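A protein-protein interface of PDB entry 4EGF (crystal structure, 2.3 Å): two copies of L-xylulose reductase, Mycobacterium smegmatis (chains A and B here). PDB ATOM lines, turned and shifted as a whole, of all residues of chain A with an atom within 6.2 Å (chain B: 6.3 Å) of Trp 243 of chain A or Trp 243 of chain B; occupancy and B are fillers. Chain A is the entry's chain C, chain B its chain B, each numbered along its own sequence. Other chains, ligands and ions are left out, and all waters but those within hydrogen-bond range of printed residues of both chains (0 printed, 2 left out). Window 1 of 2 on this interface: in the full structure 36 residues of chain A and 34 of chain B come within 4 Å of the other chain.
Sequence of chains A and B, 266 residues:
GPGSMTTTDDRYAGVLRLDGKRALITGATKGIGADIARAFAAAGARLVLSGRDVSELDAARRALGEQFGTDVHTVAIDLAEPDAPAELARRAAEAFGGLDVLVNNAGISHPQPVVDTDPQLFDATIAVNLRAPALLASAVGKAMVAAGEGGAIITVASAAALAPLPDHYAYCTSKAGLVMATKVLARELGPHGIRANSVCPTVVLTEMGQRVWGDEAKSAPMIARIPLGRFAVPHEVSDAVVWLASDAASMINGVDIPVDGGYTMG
The backbone carbonyl oxygen of Trp 243 of chain B is in hydrogen-bond range of the side-chain hydroxyl of Ser 246 of chain B (2.7 Å).
NE1 of Trp 243 of chain B is in hydrogen-bond range of O of Ala 248 of chain B (3.0 Å).
OG of Ser 246 of chain B lies close to N of Ala 248 of chain B, at 3.2 Å.
The side-chain hydroxyl of Tyr 12 of chain A sits at hydrogen-bond distance from the side-chain carboxylate of Asp 239 of chain A (2.6 Å).
The side-chain hydroxyl (OG) of Ser 246 of chain A sits close to the backbone NH (N) of Ala 248 of chain A (3.3 Å).
The backbone carbonyl oxygen of Ala 248 of chain A sits at hydrogen-bond distance from the indole nitrogen of Trp 243 of chain A (3.1 Å).
Among the printed residues, pairs that only touch across the chains: Ala 248 of chain A with Asp 239 of chain B (3.3 Å), Trp 243 of chain A with Trp 243 of chain B (3.4 Å), Asp 239 of chain A with Ala 248 of chain B (3.5 Å), Leu 16 of chain A with Leu 16 of chain B (3.6 Å) and Asp 247 of chain A with Asp 239 of chain B (3.7 Å).
Printed residues of chain B within 4 Å of Trp 243 of chain A: Trp 243.
Trp 243 of chain B touches one residue of chain A.
Of the printed residues of chain B, Ala 248 of chain A touches Asp 239 (3.3 Å).
Printed residues of chain A within 4 Å of Ala 248 of chain B: Asp 239 (3.5 Å).
Ser 246 of chain A touches none of the printed residues of chain B.
Ser 238 of chain A touches none of the printed residues of chain B.
Hydrophobic or aromatic side chains of chain A that line the printed part of chain B: Leu 16, Trp 243 and Ala 248.
Of the 18 printed residues of chain B, 4 touch a printed residue of chain A.
Among the printed residues, no Asp or Glu carboxylate lies within 4 Å of a Lys or Arg side-chain nitrogen of the other chain.
Leu 16 of chain A touches its own counterpart, Leu 16 of chain B.
Asp 239 of chain A touches Ala 248 of chain B, and with the chains exchanged Ala 248 of chain A touches Asp 239 of chain B.
Trp 243 of chain A touches its own counterpart, Trp 243 of chain B.
Asp 247 of chain A touches Asp 239 of chain B, but with the chains exchanged Asp 239 of chain A does not touch Asp 247 of chain B (4.02 Å).
Positions printed for both chains: 12, 16, 195, 238, 239, 240, 241, 242, 243, 244, 245, 246, 247, 248, 249, 252 and 257.
Of the 5 pairs that touch across the chains among the printed residues, 4 have their exchanged pair printed and touching as well.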
ATOM      1  N   TYR A  12     -31.852  10.170  14.218  1.00  0.00           N
ATOM      2  CA  TYR A  12     -30.500  10.272  13.723  1.00  0.00           C
ATOM      3  C   TYR A  12     -29.839  11.578  14.089  1.00  0.00           C
ATOM      4  O   TYR A  12     -30.144  12.615  13.514  1.00  0.00           O
ATOM      5  CB  TYR A  12     -30.529  10.085  12.211  1.00  0.00           C
ATOM      6  CG  TYR A  12     -31.321   8.864  11.822  1.00  0.00           C
ATOM      7  CD1 TYR A  12     -30.882   7.602  12.173  1.00  0.00           C
ATOM      8  CD2 TYR A  12     -32.523   8.970  11.143  1.00  0.00           C
ATOM      9  CE1 TYR A  12     -31.616   6.462  11.838  1.00  0.00           C
ATOM     10  CE2 TYR A  12     -33.261   7.842  10.802  1.00  0.00           C
ATOM     11  CZ  TYR A  12     -32.798   6.596  11.154  1.00  0.00           C
ATOM     12  OH  TYR A  12     -33.505   5.471  10.839  1.00  0.00           O
ATOM     13  N   LEU A  16     -24.544   9.833  13.307  1.00  0.00           N
ATOM     14  CA  LEU A  16     -25.577   9.434  12.339  1.00  0.00           C
ATOM     15  C   LEU A  16     -26.294  10.596  11.640  1.00  0.00           C
ATOM     16  O   LEU A  16     -27.215  10.356  10.895  1.00  0.00           O
ATOM     17  CB  LEU A  16     -26.605   8.522  13.000  1.00  0.00           C
ATOM     18  CG  LEU A  16     -26.088   7.225  13.619  1.00  0.00           C
ATOM     19  CD1 LEU A  16     -27.271   6.362  14.041  1.00  0.00           C
ATOM     20  CD2 LEU A  16     -25.217   6.510  12.619  1.00  0.00           C
ATOM     21  N   ARG A 195     -16.758   2.541   0.062  1.00  0.00           N
ATOM     22  CA  ARG A 195     -17.188   1.415   0.847  1.00  0.00           C
ATOM     23  C   ARG A 195     -18.486   0.843   0.262  1.00  0.00           C
ATOM     24  O   ARG A 195     -19.442   1.563   0.026  1.00  0.00           O
ATOM     25  CB  ARG A 195     -17.395   1.837   2.315  1.00  0.00           C
ATOM     26  CG  ARG A 195     -16.124   2.394   2.973  1.00  0.00           C
ATOM     27  CD  ARG A 195     -16.325   2.805   4.443  1.00  0.00           C
ATOM     28  NE  ARG A 195     -17.391   3.830   4.638  1.00  0.00           N
ATOM     29  CZ  ARG A 195     -18.635   3.572   5.047  1.00  0.00           C
ATOM     30  NH1 ARG A 195     -19.017   2.327   5.334  1.00  0.00           N
ATOM     31  NH2 ARG A 195     -19.505   4.557   5.195  1.00  0.00           N
ATOM     32  N   SER A 238     -33.924   0.837   7.610  1.00  0.00           N
ATOM     33  CA  SER A 238     -33.413   2.205   7.439  1.00  0.00           C
ATOM     34  C   SER A 238     -32.254   2.508   8.391  1.00  0.00           C
ATOM     35  O   SER A 238     -31.303   3.195   8.030  1.00  0.00           O
ATOM     36  CB  SER A 238     -34.525   3.227   7.651  1.00  0.00           C
ATOM     37  OG  SER A 238     -35.532   3.126   6.653  1.00  0.00           O
ATOM     38  N   ASP A 239     -32.337   1.996   9.611  1.00  0.00           N
ATOM     39  CA  ASP A 239     -31.292   2.234  10.616  1.00  0.00           C
ATOM     40  C   ASP A 239     -30.003   1.624  10.160  1.00  0.00           C
ATOM     41  O   ASP A 239     -28.968   2.226  10.286  1.00  0.00           O
ATOM     42  CB  ASP A 239     -31.638   1.593  11.963  1.00  0.00           C
ATOM     43  CG  ASP A 239     -32.752   2.300  12.706  1.00  0.00           C
ATOM     44  OD1 ASP A 239     -32.968   3.530  12.525  1.00  0.00           O
ATOM     45  OD2 ASP A 239     -33.416   1.602  13.486  1.00  0.00           O
ATOM     46  N   ALA A 240     -30.063   0.408   9.657  1.00  0.00           N
ATOM     47  CA  ALA A 240     -28.851  -0.282   9.230  1.00  0.00           C
ATOM     48  C   ALA A 240     -28.206   0.448   8.046  1.00  0.00           C
ATOM     49  O   ALA A 240     -26.981   0.550   7.966  1.00  0.00           O
ATOM     50  CB  ALA A 240     -29.142  -1.751   8.898  1.00  0.00           C
ATOM     51  N   VAL A 241     -29.045   0.978   7.153  1.00  0.00           N
ATOM     52  CA  VAL A 241     -28.553   1.750   6.004  1.00  0.00           C
ATOM     53  C   VAL A 241     -27.930   3.097   6.434  1.00  0.00           C
ATOM     54  O   VAL A 241     -26.860   3.466   5.951  1.00  0.00           O
ATOM     55  CB  VAL A 241     -29.646   1.993   4.948  1.00  0.00           C
ATOM     56  CG1 VAL A 241     -29.120   2.928   3.854  1.00  0.00           C
ATOM     57  CG2 VAL A 241     -30.119   0.674   4.355  1.00  0.00           C
ATOM     58  N   VAL A 242     -28.608   3.828   7.321  1.00  0.00           N
ATOM     59  CA  VAL A 242     -28.049   5.061   7.823  1.00  0.00           C
ATOM     60  C   VAL A 242     -26.713   4.775   8.507  1.00  0.00           C
ATOM     61  O   VAL A 242     -25.713   5.482   8.310  1.00  0.00           O
ATOM     62  CB  VAL A 242     -28.963   5.764   8.836  1.00  0.00           C
ATOM     63  CG1 VAL A 242     -28.222   6.920   9.466  1.00  0.00           C
ATOM     64  CG2 VAL A 242     -30.267   6.249   8.183  1.00  0.00           C
ATOM     65  N   TRP A 243     -26.686   3.743   9.325  1.00  0.00           N
ATOM     66  CA  TRP A 243     -25.456   3.422  10.027  1.00  0.00           C
ATOM     67  C   TRP A 243     -24.325   3.200   9.015  1.00  0.00           C
ATOM     68  O   TRP A 243     -23.251   3.745   9.164  1.00  0.00           O
ATOM     69  CB  TRP A 243     -25.649   2.220  10.988  1.00  0.00           C
ATOM     70  CG  TRP A 243     -24.321   1.735  11.498  1.00  0.00           C
ATOM     71  CD1 TRP A 243     -23.425   2.424  12.292  1.00  0.00           C
ATOM     72  CD2 TRP A 243     -23.666   0.455  11.199  1.00  0.00           C
ATOM     73  NE1 TRP A 243     -22.275   1.680  12.499  1.00  0.00           N
ATOM     74  CE2 TRP A 243     -22.373   0.484  11.879  1.00  0.00           C
ATOM     75  CE3 TRP A 243     -24.021  -0.666  10.474  1.00  0.00           C
ATOM     76  CZ2 TRP A 243     -21.485  -0.568  11.813  1.00  0.00           C
ATOM     77  CZ3 TRP A 243     -23.124  -1.730  10.412  1.00  0.00           C
ATOM     78  CH2 TRP A 243     -21.879  -1.679  11.055  1.00  0.00           C
ATOM     79  N   LEU A 244     -24.570   2.411   7.976  1.00  0.00           N
ATOM     80  CA  LEU A 244     -23.553   2.065   6.980  1.00  0.00           C
ATOM     81  C   LEU A 244     -23.081   3.293   6.213  1.00  0.00           C
ATOM     82  O   LEU A 244     -21.919   3.383   5.800  1.00  0.00           O
ATOM     83  CB  LEU A 244     -24.123   1.034   6.014  1.00  0.00           C
ATOM     84  CG  LEU A 244     -24.114  -0.438   6.462  1.00  0.00           C
ATOM     85  CD1 LEU A 244     -24.875  -1.281   5.476  1.00  0.00           C
ATOM     86  CD2 LEU A 244     -22.690  -0.995   6.654  1.00  0.00           C
ATOM     87  N   ALA A 245     -23.979   4.247   6.004  1.00  0.00           N
ATOM     88  CA  ALA A 245     -23.631   5.505   5.332  1.00  0.00           C
ATOM     89  C   ALA A 245     -22.784   6.430   6.209  1.00  0.00           C
ATOM     90  O   ALA A 245     -22.123   7.337   5.693  1.00  0.00           O
ATOM     91  CB  ALA A 245     -24.881   6.232   4.919  1.00  0.00           C
ATOM     92  N   SER A 246     -22.839   6.216   7.528  1.00  0.00           N
ATOM     93  CA  SER A 246     -22.235   7.142   8.518  1.00  0.00           C
ATOM     94  C   SER A 246     -20.724   6.939   8.729  1.00  0.00           C
ATOM     95  O   SER A 246     -20.160   5.928   8.306  1.00  0.00           O
ATOM     96  CB  SER A 246     -22.958   7.002   9.867  1.00  0.00           C
ATOM     97  OG  SER A 246     -22.662   5.783  10.506  1.00  0.00           O
ATOM     98  N   ASP A 247     -20.085   7.875   9.415  1.00  0.00           N
ATOM     99  CA  ASP A 247     -18.668   7.695   9.805  1.00  0.00           C
ATOM    100  C   ASP A 247     -18.487   6.657  10.929  1.00  0.00           C
ATOM    101  O   ASP A 247     -17.340   6.271  11.250  1.00  0.00           O
ATOM    102  CB  ASP A 247     -18.062   9.018  10.271  1.00  0.00           C
ATOM    103  CG  ASP A 247     -17.968  10.059   9.148  1.00  0.00           C
ATOM    104  OD1 ASP A 247     -18.054   9.724   7.926  1.00  0.00           O
ATOM    105  OD2 ASP A 247     -17.798  11.237   9.507  1.00  0.00           O
ATOM    106  N   ALA A 248     -19.608   6.251  11.553  1.00  0.00           N
ATOM    107  CA  ALA A 248     -19.610   5.167  12.515  1.00  0.00           C
ATOM    108  C   ALA A 248     -19.453   3.775  11.834  1.00  0.00           C
ATOM    109  O   ALA A 248     -19.389   2.748  12.519  1.00  0.00           O
ATOM    110  CB  ALA A 248     -20.855   5.218  13.380  1.00  0.00           C
ATOM    111  N   ALA A 249     -19.398   3.755  10.509  1.00  0.00           N
ATOM    112  CA  ALA A 249     -19.112   2.538   9.760  1.00  0.00           C
ATOM    113  C   ALA A 249     -17.871   2.706   8.861  1.00  0.00           C
ATOM    114  O   ALA A 249     -17.716   1.995   7.872  1.00  0.00           O
ATOM    115  CB  ALA A 249     -20.329   2.127   8.925  1.00  0.00           C
ATOM    116  N   ILE A 252     -16.038  -0.367   7.680  1.00  0.00           N
ATOM    117  CA  ILE A 252     -16.902  -1.442   7.269  1.00  0.00           C
ATOM    118  C   ILE A 252     -16.932  -1.495   5.757  1.00  0.00           C
ATOM    119  O   ILE A 252     -17.506  -0.625   5.119  1.00  0.00           O
ATOM    120  CB  ILE A 252     -18.354  -1.245   7.791  1.00  0.00           C
ATOM    121  CG1 ILE A 252     -18.367  -1.042   9.309  1.00  0.00           C
ATOM    122  CG2 ILE A 252     -19.210  -2.455   7.379  1.00  0.00           C
ATOM    123  CD1 ILE A 252     -17.656  -2.139  10.095  1.00  0.00           C
ATOM    124  N   ILE A 257     -25.029  -7.508   6.034  1.00  0.00           N
ATOM    125  CA  ILE A 257     -25.614  -7.386   7.369  1.00  0.00           C
ATOM    126  C   ILE A 257     -27.001  -7.958   7.291  1.00  0.00           C
ATOM    127  O   ILE A 257     -27.892  -7.353   6.736  1.00  0.00           O
ATOM    128  CB  ILE A 257     -25.659  -5.955   7.864  1.00  0.00           C
ATOM    129  CG1 ILE A 257     -24.238  -5.430   8.035  1.00  0.00           C
ATOM    130  CG2 ILE A 257     -26.370  -5.875   9.213  1.00  0.00           C
ATOM    131  CD1 ILE A 257     -24.174  -3.959   7.880  1.00  0.00           C
ATOM    132  N   TYR B  12     -22.380   9.912  20.070  1.00  0.00           N
ATOM    133  CA  TYR B  12     -23.540   9.050  20.234  1.00  0.00           C
ATOM    134  C   TYR B  12     -24.733   9.837  20.771  1.00  0.00           C
ATOM    135  O   TYR B  12     -24.716  10.340  21.907  1.00  0.00           O
ATOM    136  CB  TYR B  12     -23.158   7.887  21.157  1.00  0.00           C
ATOM    137  CG  TYR B  12     -21.868   7.211  20.695  1.00  0.00           C
ATOM    138  CD1 TYR B  12     -21.840   6.439  19.526  1.00  0.00           C
ATOM    139  CD2 TYR B  12     -20.675   7.394  21.367  1.00  0.00           C
ATOM    140  CE1 TYR B  12     -20.658   5.826  19.082  1.00  0.00           C
ATOM    141  CE2 TYR B  12     -19.500   6.793  20.927  1.00  0.00           C
ATOM    142  CZ  TYR B  12     -19.508   6.011  19.790  1.00  0.00           C
ATOM    143  OH  TYR B  12     -18.379   5.418  19.365  1.00  0.00           O
ATOM    144  N   LEU B  16     -28.551   6.148  19.253  1.00  0.00           N
ATOM    145  CA  LEU B  16     -27.321   5.595  19.745  1.00  0.00           C
ATOM    146  C   LEU B  16     -27.032   6.008  21.167  1.00  0.00           C
ATOM    147  O   LEU B  16     -25.919   5.748  21.667  1.00  0.00           O
ATOM    148  CB  LEU B  16     -26.131   6.010  18.848  1.00  0.00           C
ATOM    149  CG  LEU B  16     -26.068   5.457  17.430  1.00  0.00           C
ATOM    150  CD1 LEU B  16     -24.774   5.886  16.740  1.00  0.00           C
ATOM    151  CD2 LEU B  16     -26.224   3.948  17.482  1.00  0.00           C
ATOM    152  N   ARG B 195     -30.283 -10.524  22.250  1.00  0.00           N
ATOM    153  CA  ARG B 195     -29.606 -10.490  20.940  1.00  0.00           C
ATOM    154  C   ARG B 195     -28.129 -10.675  21.165  1.00  0.00           C
ATOM    155  O   ARG B 195     -27.507  -9.939  21.958  1.00  0.00           O
ATOM    156  CB  ARG B 195     -29.811  -9.151  20.208  1.00  0.00           C
ATOM    157  CG  ARG B 195     -31.231  -8.887  19.752  1.00  0.00           C
ATOM    158  CD  ARG B 195     -31.445  -7.585  19.031  1.00  0.00           C
ATOM    159  NE  ARG B 195     -30.997  -6.439  19.807  1.00  0.00           N
ATOM    160  CZ  ARG B 195     -29.780  -5.873  19.716  1.00  0.00           C
ATOM    161  NH1 ARG B 195     -28.855  -6.326  18.881  1.00  0.00           N
ATOM    162  NH2 ARG B 195     -29.486  -4.835  20.464  1.00  0.00           N
ATOM    163  N   SER B 238     -15.396   0.385  18.522  1.00  0.00           N
ATOM    164  CA  SER B 238     -16.367   0.883  19.506  1.00  0.00           C
ATOM    165  C   SER B 238     -17.687   1.338  18.870  1.00  0.00           C
ATOM    166  O   SER B 238     -18.752   1.042  19.409  1.00  0.00           O
ATOM    167  CB  SER B 238     -15.769   2.027  20.340  1.00  0.00           C
ATOM    168  OG  SER B 238     -14.635   1.593  21.099  1.00  0.00           O
ATOM    169  N   ASP B 239     -17.613   2.076  17.744  1.00  0.00           N
ATOM    170  CA  ASP B 239     -18.813   2.438  16.971  1.00  0.00           C
ATOM    171  C   ASP B 239     -19.747   1.230  16.698  1.00  0.00           C
ATOM    172  O   ASP B 239     -20.981   1.301  16.825  1.00  0.00           O
ATOM    173  CB  ASP B 239     -18.402   3.027  15.623  1.00  0.00           C
ATOM    174  CG  ASP B 239     -17.867   4.491  15.720  1.00  0.00           C
ATOM    175  OD1 ASP B 239     -18.127   5.196  16.729  1.00  0.00           O
ATOM    176  OD2 ASP B 239     -17.197   4.935  14.750  1.00  0.00           O
ATOM    177  N   ALA B 240     -19.148   0.133  16.282  1.00  0.00           N
ATOM    178  CA  ALA B 240     -19.893  -1.001  15.827  1.00  0.00           C
ATOM    179  C   ALA B 240     -20.569  -1.645  17.033  1.00  0.00           C
ATOM    180  O   ALA B 240     -21.717  -2.160  16.926  1.00  0.00           O
ATOM    181  CB  ALA B 240     -18.992  -1.991  15.129  1.00  0.00           C
ATOM    182  N   VAL B 241     -19.872  -1.602  18.175  1.00  0.00           N
ATOM    183  CA  VAL B 241     -20.395  -2.182  19.401  1.00  0.00           C
ATOM    184  C   VAL B 241     -21.554  -1.360  19.929  1.00  0.00           C
ATOM    185  O   VAL B 241     -22.604  -1.928  20.321  1.00  0.00           O
ATOM    186  CB  VAL B 241     -19.324  -2.307  20.464  1.00  0.00           C
ATOM    187  CG1 VAL B 241     -19.959  -2.635  21.812  1.00  0.00           C
ATOM    188  CG2 VAL B 241     -18.308  -3.367  20.040  1.00  0.00           C
ATOM    189  N   VAL B 242     -21.402  -0.032  19.886  1.00  0.00           N
ATOM    190  CA  VAL B 242     -22.477   0.862  20.364  1.00  0.00           C
ATOM    191  C   VAL B 242     -23.705   0.637  19.509  1.00  0.00           C
ATOM    192  O   VAL B 242     -24.808   0.493  20.026  1.00  0.00           O
ATOM    193  CB  VAL B 242     -22.094   2.361  20.375  1.00  0.00           C
ATOM    194  CG1 VAL B 242     -23.303   3.215  20.688  1.00  0.00           C
ATOM    195  CG2 VAL B 242     -20.929   2.655  21.340  1.00  0.00           C
ATOM    196  N   TRP B 243     -23.497   0.560  18.198  1.00  0.00           N
ATOM    197  CA  TRP B 243     -24.606   0.331  17.261  1.00  0.00           C
ATOM    198  C   TRP B 243     -25.326  -0.954  17.618  1.00  0.00           C
ATOM    199  O   TRP B 243     -26.576  -0.969  17.716  1.00  0.00           O
ATOM    200  CB  TRP B 243     -24.118   0.322  15.812  1.00  0.00           C
ATOM    201  CG  TRP B 243     -25.178  -0.090  14.845  1.00  0.00           C
ATOM    202  CD1 TRP B 243     -26.390   0.557  14.565  1.00  0.00           C
ATOM    203  CD2 TRP B 243     -25.220  -1.303  14.045  1.00  0.00           C
ATOM    204  NE1 TRP B 243     -27.130  -0.169  13.669  1.00  0.00           N
ATOM    205  CE2 TRP B 243     -26.475  -1.272  13.310  1.00  0.00           C
ATOM    206  CE3 TRP B 243     -24.363  -2.351  13.849  1.00  0.00           C
ATOM    207  CZ2 TRP B 243     -26.826  -2.246  12.453  1.00  0.00           C
ATOM    208  CZ3 TRP B 243     -24.739  -3.349  12.953  1.00  0.00           C
ATOM    209  CH2 TRP B 243     -25.949  -3.294  12.287  1.00  0.00           C
ATOM    210  N   LEU B 244     -24.565  -2.041  17.832  1.00  0.00           N
ATOM    211  CA  LEU B 244     -25.153  -3.369  18.133  1.00  0.00           C
ATOM    212  C   LEU B 244     -25.937  -3.381  19.478  1.00  0.00           C
ATOM    213  O   LEU B 244     -26.978  -4.104  19.630  1.00  0.00           O
ATOM    214  CB  LEU B 244     -24.065  -4.450  18.129  1.00  0.00           C
ATOM    215  CG  LEU B 244     -23.671  -4.959  16.741  1.00  0.00           C
ATOM    216  CD1 LEU B 244     -22.342  -5.700  16.761  1.00  0.00           C
ATOM    217  CD2 LEU B 244     -24.814  -5.864  16.221  1.00  0.00           C
ATOM    218  N   ALA B 245     -25.432  -2.602  20.438  1.00  0.00           N
ATOM    219  CA  ALA B 245     -26.103  -2.413  21.701  1.00  0.00           C
ATOM    220  C   ALA B 245     -27.396  -1.599  21.560  1.00  0.00           C
ATOM    221  O   ALA B 245     -28.312  -1.822  22.313  1.00  0.00           O
ATOM    222  CB  ALA B 245     -25.187  -1.737  22.696  1.00  0.00           C
ATOM    223  N   SER B 246     -27.464  -0.679  20.592  1.00  0.00           N
ATOM    224  CA  SER B 246     -28.588   0.279  20.482  1.00  0.00           C
ATOM    225  C   SER B 246     -29.869  -0.313  19.885  1.00  0.00           C
ATOM    226  O   SER B 246     -29.892  -1.447  19.395  1.00  0.00           O
ATOM    227  CB  SER B 246     -28.168   1.514  19.640  1.00  0.00           C
ATOM    228  OG  SER B 246     -28.066   1.236  18.257  1.00  0.00           O
ATOM    229  N   ASP B 247     -30.919   0.484  19.890  1.00  0.00           N
ATOM    230  CA  ASP B 247     -32.182   0.081  19.265  1.00  0.00           C
ATOM    231  C   ASP B 247     -32.164   0.230  17.743  1.00  0.00           C
ATOM    232  O   ASP B 247     -33.123  -0.175  17.082  1.00  0.00           O
ATOM    233  CB  ASP B 247     -33.345   0.881  19.858  1.00  0.00           C
ATOM    234  CG  ASP B 247     -33.623   0.504  21.271  1.00  0.00           C
ATOM    235  OD1 ASP B 247     -33.500  -0.705  21.625  1.00  0.00           O
ATOM    236  OD2 ASP B 247     -33.975   1.411  22.042  1.00  0.00           O
ATOM    237  N   ALA B 248     -31.079   0.810  17.208  1.00  0.00           N
ATOM    238  CA  ALA B 248     -30.775   0.804  15.760  1.00  0.00           C
ATOM    239  C   ALA B 248     -30.319  -0.585  15.244  1.00  0.00           C
ATOM    240  O   ALA B 248     -30.062  -0.761  14.032  1.00  0.00           O
ATOM    241  CB  ALA B 248     -29.718   1.877  15.427  1.00  0.00           C
ATOM    242  N   ALA B 249     -30.186  -1.550  16.160  1.00  0.00           N
ATOM    243  CA  ALA B 249     -29.879  -2.960  15.822  1.00  0.00           C
ATOM    244  C   ALA B 249     -30.933  -3.943  16.417  1.00  0.00           C
ATOM    245  O   ALA B 249     -30.620  -5.072  16.742  1.00  0.00           O
ATOM    246  CB  ALA B 249     -28.483  -3.321  16.270  1.00  0.00           C
ATOM    247  N   SER B 250     -32.171  -3.481  16.534  1.00  0.00           N
ATOM    248  CA  SER B 250     -33.222  -4.231  17.220  1.00  0.00           C
ATOM    249  C   SER B 250     -33.601  -5.579  16.537  1.00  0.00           C
ATOM    250  O   SER B 250     -34.059  -6.495  17.213  1.00  0.00           O
ATOM    251  CB  SER B 250     -34.472  -3.330  17.455  1.00  0.00           C
ATOM    252  OG  SER B 250     -34.861  -2.617  16.267  1.00  0.00           O
ATOM    253  N   ILE B 252     -31.089  -7.252  14.814  1.00  0.00           N
ATOM    254  CA  ILE B 252     -29.781  -7.853  14.510  1.00  0.00           C
ATOM    255  C   ILE B 252     -29.427  -8.906  15.537  1.00  0.00           C
ATOM    256  O   ILE B 252     -29.267  -8.610  16.698  1.00  0.00           O
ATOM    257  CB  ILE B 252     -28.674  -6.777  14.464  1.00  0.00           C
ATOM    258  CG1 ILE B 252     -29.114  -5.591  13.586  1.00  0.00           C
ATOM    259  CG2 ILE B 252     -27.369  -7.369  13.982  1.00  0.00           C
ATOM    260  CD1 ILE B 252     -29.421  -5.970  12.139  1.00  0.00           C
ATOM    261  N   ILE B 257     -20.034  -8.980  12.524  1.00  0.00           N
ATOM    262  CA  ILE B 257     -19.688  -7.828  11.773  1.00  0.00           C
ATOM    263  C   ILE B 257     -18.179  -7.682  11.692  1.00  0.00           C
ATOM    264  O   ILE B 257     -17.602  -7.340  12.657  1.00  0.00           O
ATOM    265  CB  ILE B 257     -20.305  -6.576  12.406  1.00  0.00           C
ATOM    266  CG1 ILE B 257     -21.811  -6.582  12.084  1.00  0.00           C
ATOM    267  CG2 ILE B 257     -19.611  -5.312  11.871  1.00  0.00           C
ATOM    268  CD1 ILE B 257     -22.638  -6.192  13.251  1.00  0.00           C
